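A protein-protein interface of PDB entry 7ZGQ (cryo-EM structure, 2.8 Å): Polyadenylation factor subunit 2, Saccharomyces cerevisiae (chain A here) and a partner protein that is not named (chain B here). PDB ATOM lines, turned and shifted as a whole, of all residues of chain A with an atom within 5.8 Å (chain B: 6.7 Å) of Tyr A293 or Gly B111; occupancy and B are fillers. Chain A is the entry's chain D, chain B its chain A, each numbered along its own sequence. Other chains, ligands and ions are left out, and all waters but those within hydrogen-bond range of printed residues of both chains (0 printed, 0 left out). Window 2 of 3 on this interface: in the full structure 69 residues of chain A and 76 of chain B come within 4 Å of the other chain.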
ATOM      1  N   ASP A 290     -16.574 -13.453 -28.279  1.00  0.00           N
ATOM      2  CA  ASP A 290     -15.828 -13.630 -27.037  1.00  0.00           C
ATOM      3  C   ASP A 290     -15.376 -15.083 -26.956  1.00  0.00           C
ATOM      4  O   ASP A 290     -16.191 -15.981 -26.724  1.00  0.00           O
ATOM      5  CB  ASP A 290     -16.685 -13.250 -25.831  1.00  0.00           C
ATOM      6  CG  ASP A 290     -15.854 -12.892 -24.614  1.00  0.00           C
ATOM      7  OD1 ASP A 290     -14.858 -13.592 -24.341  1.00  0.00           O
ATOM      8  OD2 ASP A 290     -16.200 -11.907 -23.928  1.00  0.00           O
ATOM      9  N   ILE A 291     -14.076 -15.314 -27.149  1.00  0.00           N
ATOM     10  CA  ILE A 291     -13.561 -16.677 -27.165  1.00  0.00           C
ATOM     11  C   ILE A 291     -13.601 -17.318 -25.786  1.00  0.00           C
ATOM     12  O   ILE A 291     -13.459 -18.542 -25.673  1.00  0.00           O
ATOM     13  CB  ILE A 291     -12.128 -16.709 -27.729  1.00  0.00           C
ATOM     14  CG1 ILE A 291     -11.110 -16.385 -26.635  1.00  0.00           C
ATOM     15  CG2 ILE A 291     -11.995 -15.737 -28.890  1.00  0.00           C
ATOM     16  CD1 ILE A 291      -9.716 -16.148 -27.156  1.00  0.00           C
ATOM     17  N   ARG A 292     -13.789 -16.526 -24.729  1.00  0.00           N
ATOM     18  CA  ARG A 292     -13.782 -17.077 -23.378  1.00  0.00           C
ATOM     19  C   ARG A 292     -14.947 -18.034 -23.157  1.00  0.00           C
ATOM     20  O   ARG A 292     -14.791 -19.068 -22.496  1.00  0.00           O
ATOM     21  CB  ARG A 292     -13.808 -15.946 -22.351  1.00  0.00           C
ATOM     22  CG  ARG A 292     -12.432 -15.539 -21.851  1.00  0.00           C
ATOM     23  CD  ARG A 292     -12.501 -14.294 -20.986  1.00  0.00           C
ATOM     24  NE  ARG A 292     -13.007 -13.147 -21.729  1.00  0.00           N
ATOM     25  CZ  ARG A 292     -13.422 -12.017 -21.172  1.00  0.00           C
ATOM     26  NH1 ARG A 292     -13.407 -11.847 -19.861  1.00  0.00           N
ATOM     27  NH2 ARG A 292     -13.863 -11.035 -21.951  1.00  0.00           N
ATOM     28  N   TYR A 293     -16.123 -17.712 -23.693  1.00  0.00           N
ATOM     29  CA  TYR A 293     -17.315 -18.540 -23.513  1.00  0.00           C
ATOM     30  C   TYR A 293     -17.811 -19.013 -24.877  1.00  0.00           C
ATOM     31  O   TYR A 293     -18.730 -18.427 -25.448  1.00  0.00           O
ATOM     32  CB  TYR A 293     -18.410 -17.766 -22.759  1.00  0.00           C
ATOM     33  CG  TYR A 293     -17.903 -16.608 -21.929  1.00  0.00           C
ATOM     34  CD1 TYR A 293     -17.189 -16.825 -20.758  1.00  0.00           C
ATOM     35  CD2 TYR A 293     -18.149 -15.298 -22.313  1.00  0.00           C
ATOM     36  CE1 TYR A 293     -16.728 -15.768 -19.997  1.00  0.00           C
ATOM     37  CE2 TYR A 293     -17.694 -14.235 -21.558  1.00  0.00           C
ATOM     38  CZ  TYR A 293     -16.984 -14.475 -20.400  1.00  0.00           C
ATOM     39  OH  TYR A 293     -16.529 -13.417 -19.648  1.00  0.00           O
ATOM     40  N   SER A 294     -17.214 -20.097 -25.369  1.00  0.00           N
ATOM     41  CA  SER A 294     -17.676 -20.841 -26.546  1.00  0.00           C
ATOM     42  C   SER A 294     -18.125 -19.920 -27.682  1.00  0.00           C
ATOM     43  O   SER A 294     -19.277 -19.941 -28.118  1.00  0.00           O
ATOM     44  CB  SER A 294     -18.794 -21.810 -26.164  1.00  0.00           C
ATOM     45  OG  SER A 294     -19.828 -21.151 -25.455  1.00  0.00           O
ATOM     46  N   MET A 295     -17.183 -19.106 -28.160  1.00  0.00           N
ATOM     47  CA  MET A 295     -17.412 -18.225 -29.307  1.00  0.00           C
ATOM     48  C   MET A 295     -18.620 -17.317 -29.087  1.00  0.00           C
ATOM     49  O   MET A 295     -19.436 -17.106 -29.987  1.00  0.00           O
ATOM     50  CB  MET A 295     -17.584 -19.034 -30.595  1.00  0.00           C
ATOM     51  CG  MET A 295     -16.310 -19.305 -31.381  1.00  0.00           C
ATOM     52  SD  MET A 295     -15.070 -18.003 -31.282  1.00  0.00           S
ATOM     53  CE  MET A 295     -13.940 -18.726 -30.100  1.00  0.00           C
ATOM     54  N   LYS A 296     -18.740 -16.777 -27.877  1.00  0.00           N
ATOM     55  CA  LYS A 296     -19.899 -15.959 -27.541  1.00  0.00           C
ATOM     56  C   LYS A 296     -19.914 -14.683 -28.371  1.00  0.00           C
ATOM     57  O   LYS A 296     -19.013 -13.846 -28.260  1.00  0.00           O
ATOM     58  CB  LYS A 296     -19.894 -15.621 -26.051  1.00  0.00           C
ATOM     59  CG  LYS A 296     -21.218 -15.081 -25.535  1.00  0.00           C
ATOM     60  CD  LYS A 296     -22.391 -15.883 -26.078  1.00  0.00           C
ATOM     61  CE  LYS A 296     -23.715 -15.209 -25.758  1.00  0.00           C
ATOM     62  NZ  LYS A 296     -24.822 -15.735 -26.604  1.00  0.00           N
ATOM     63  N   LEU A 298     -20.931 -11.039 -29.224  1.00  0.00           N
ATOM     64  CA  LEU A 298     -21.270  -9.871 -28.424  1.00  0.00           C
ATOM     65  C   LEU A 298     -21.892  -8.741 -29.226  1.00  0.00           C
ATOM     66  O   LEU A 298     -22.731  -8.014 -28.693  1.00  0.00           O
ATOM     67  CB  LEU A 298     -20.024  -9.341 -27.705  1.00  0.00           C
ATOM     68  CG  LEU A 298     -19.088 -10.412 -27.147  1.00  0.00           C
ATOM     69  CD1 LEU A 298     -17.771  -9.800 -26.706  1.00  0.00           C
ATOM     70  CD2 LEU A 298     -19.752 -11.151 -25.997  1.00  0.00           C
ATOM     71  N   GLU B 106     -12.184 -11.281  -7.181  1.00  0.00           N
ATOM     72  CA  GLU B 106     -11.370 -10.950  -8.347  1.00  0.00           C
ATOM     73  C   GLU B 106     -11.658 -11.882  -9.518  1.00  0.00           C
ATOM     74  O   GLU B 106     -11.884 -11.418 -10.641  1.00  0.00           O
ATOM     75  CB  GLU B 106      -9.887 -10.992  -7.982  1.00  0.00           C
ATOM     76  CG  GLU B 106      -8.967 -11.205  -9.173  1.00  0.00           C
ATOM     77  CD  GLU B 106      -7.789 -10.255  -9.177  1.00  0.00           C
ATOM     78  OE1 GLU B 106      -7.362  -9.829  -8.084  1.00  0.00           O
ATOM     79  OE2 GLU B 106      -7.289  -9.932 -10.274  1.00  0.00           O
ATOM     80  N   GLY B 107     -11.653 -13.193  -9.277  1.00  0.00           N
ATOM     81  CA  GLY B 107     -11.889 -14.133 -10.361  1.00  0.00           C
ATOM     82  C   GLY B 107     -13.271 -13.994 -10.967  1.00  0.00           C
ATOM     83  O   GLY B 107     -13.437 -14.081 -12.185  1.00  0.00           O
ATOM     84  N   LYS B 108     -14.281 -13.775 -10.124  1.00  0.00           N
ATOM     85  CA  LYS B 108     -15.637 -13.596 -10.631  1.00  0.00           C
ATOM     86  C   LYS B 108     -15.777 -12.273 -11.374  1.00  0.00           C
ATOM     87  O   LYS B 108     -16.576 -12.161 -12.312  1.00  0.00           O
ATOM     88  CB  LYS B 108     -16.637 -13.683  -9.480  1.00  0.00           C
ATOM     89  CG  LYS B 108     -17.931 -14.395  -9.830  1.00  0.00           C
ATOM     90  CD  LYS B 108     -18.445 -15.212  -8.657  1.00  0.00           C
ATOM     91  CE  LYS B 108     -19.764 -15.886  -8.989  1.00  0.00           C
ATOM     92  NZ  LYS B 108     -19.768 -16.446 -10.368  1.00  0.00           N
ATOM     93  N   PHE B 109     -15.020 -11.253 -10.961  1.00  0.00           N
ATOM     94  CA  PHE B 109     -15.012  -9.990 -11.694  1.00  0.00           C
ATOM     95  C   PHE B 109     -14.449 -10.178 -13.097  1.00  0.00           C
ATOM     96  O   PHE B 109     -14.998  -9.659 -14.075  1.00  0.00           O
ATOM     97  CB  PHE B 109     -14.196  -8.943 -10.935  1.00  0.00           C
ATOM     98  CG  PHE B 109     -14.959  -8.240  -9.853  1.00  0.00           C
ATOM     99  CD1 PHE B 109     -16.217  -8.670  -9.478  1.00  0.00           C
ATOM    100  CD2 PHE B 109     -14.412  -7.145  -9.210  1.00  0.00           C
ATOM    101  CE1 PHE B 109     -16.915  -8.020  -8.481  1.00  0.00           C
ATOM    102  CE2 PHE B 109     -15.105  -6.492  -8.213  1.00  0.00           C
ATOM    103  CZ  PHE B 109     -16.358  -6.929  -7.848  1.00  0.00           C
ATOM    104  N   LYS B 110     -13.344 -10.917 -13.211  1.00  0.00           N
ATOM    105  CA  LYS B 110     -12.731 -11.144 -14.515  1.00  0.00           C
ATOM    106  C   LYS B 110     -13.613 -12.007 -15.407  1.00  0.00           C
ATOM    107  O   LYS B 110     -13.519 -11.920 -16.637  1.00  0.00           O
ATOM    108  CB  LYS B 110     -11.358 -11.790 -14.341  1.00  0.00           C
ATOM    109  CG  LYS B 110     -10.241 -10.804 -14.040  1.00  0.00           C
ATOM    110  CD  LYS B 110      -9.075 -11.489 -13.346  1.00  0.00           C
ATOM    111  CE  LYS B 110      -8.108 -12.090 -14.350  1.00  0.00           C
ATOM    112  NZ  LYS B 110      -7.207 -11.062 -14.937  1.00  0.00           N
ATOM    113  N   GLY B 111     -14.469 -12.837 -14.814  1.00  0.00           N
ATOM    114  CA  GLY B 111     -15.328 -13.712 -15.590  1.00  0.00           C
ATOM    115  C   GLY B 111     -16.430 -13.004 -16.348  1.00  0.00           C
ATOM    116  O   GLY B 111     -16.986 -13.591 -17.282  1.00  0.00           O
ATOM    117  N   LYS B 112     -16.759 -11.770 -15.974  1.00  0.00           N
ATOM    118  CA  LYS B 112     -17.769 -10.990 -16.678  1.00  0.00           C
ATOM    119  C   LYS B 112     -17.285  -9.564 -16.893  1.00  0.00           C
ATOM    120  O   LYS B 112     -18.034  -8.599 -16.720  1.00  0.00           O
ATOM    121  CB  LYS B 112     -19.103 -11.006 -15.931  1.00  0.00           C
ATOM    122  CG  LYS B 112     -19.000 -10.700 -14.451  1.00  0.00           C
ATOM    123  CD  LYS B 112     -19.909 -11.613 -13.652  1.00  0.00           C
ATOM    124  CE  LYS B 112     -21.371 -11.288 -13.906  1.00  0.00           C
ATOM    125  NZ  LYS B 112     -22.251 -11.780 -12.814  1.00  0.00           N
ATOM    126  N   SER B 113     -16.020  -9.416 -17.275  1.00  0.00           N
ATOM    127  CA  SER B 113     -15.440  -8.122 -17.608  1.00  0.00           C
ATOM    128  C   SER B 113     -14.921  -8.168 -19.037  1.00  0.00           C
ATOM    129  O   SER B 113     -14.118  -9.041 -19.382  1.00  0.00           O
ATOM    130  CB  SER B 113     -14.310  -7.755 -16.644  1.00  0.00           C
ATOM    131  OG  SER B 113     -13.909  -6.408 -16.819  1.00  0.00           O
ATOM    132  N   LEU B 114     -15.384  -7.230 -19.864  1.00  0.00           N
ATOM    133  CA  LEU B 114     -14.920  -7.177 -21.244  1.00  0.00           C
ATOM    134  C   LEU B 114     -13.495  -6.648 -21.336  1.00  0.00           C
ATOM    135  O   LEU B 114     -12.734  -7.069 -22.214  1.00  0.00           O
ATOM    136  CB  LEU B 114     -15.859  -6.309 -22.080  1.00  0.00           C
ATOM    137  CG  LEU B 114     -16.853  -7.039 -22.982  1.00  0.00           C
ATOM    138  CD1 LEU B 114     -16.119  -7.928 -23.962  1.00  0.00           C
ATOM    139  CD2 LEU B 114     -17.842  -7.845 -22.157  1.00  0.00           C
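The guanidinium group (NH1) of Arg A292 is in hydrogen-bond range of the backbone carbonyl oxygen (O) of Lys B110 (3.2 Å). OH of Tyr A293 is in hydrogen-bond range of O of Gly B111 (2.4 Å). The guanidinium group (NH1) of Arg A292 lies within hydrogen-bond range of the backbone carbonyl oxygen (O) of Ser B113.
The side-chain carboxylate (OD2) of Asp A290 is in salt-bridge range of the guanidinium group (NH2) of Arg A292. O of Lys A296 lies within hydrogen-bond range of N of Asp A290 (2.5 Å).
Asp A290 touches Leu B114. CD1 of Leu A298 touches CD1 of Leu B114 (3.7 Å).
Of the printed residues of chain B, Tyr A293 touches Gly B111 (2.4 Å). Gly B111 touches just one residue of chain A: Tyr A293 (2.4 Å). Of the printed residues of chain A, Ser B113 touches Arg A292 (2.9 Å). Of the printed residues of chain B, Leu A298 touches Leu B114 (3.7 Å). Phe B109 touches none of the printed residues of chain A. Lys B108 touches none of the printed residues of chain A. The nearest printed residue of chain A that does not touch Ser B113 is Tyr A293 (4.7 Å).
Printed residues of chain B that touch a printed residue of chain A: Lys B110, Gly B111, Ser B113 and Leu B114. Printed residues of chain A that touch a printed residue of chain B: Asp A290, Arg A292, Tyr A293 and Leu A298. Hydrophobic or aromatic side chains of chain A that line the printed part of chain B: Tyr A293 and Leu A298. Among the printed residues, 5 pairs touch across the chains. Among the printed residues, no Asp or Glu carboxylate lies within 4 Å of a Lys or Arg side-chain nitrogen of the other chain.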
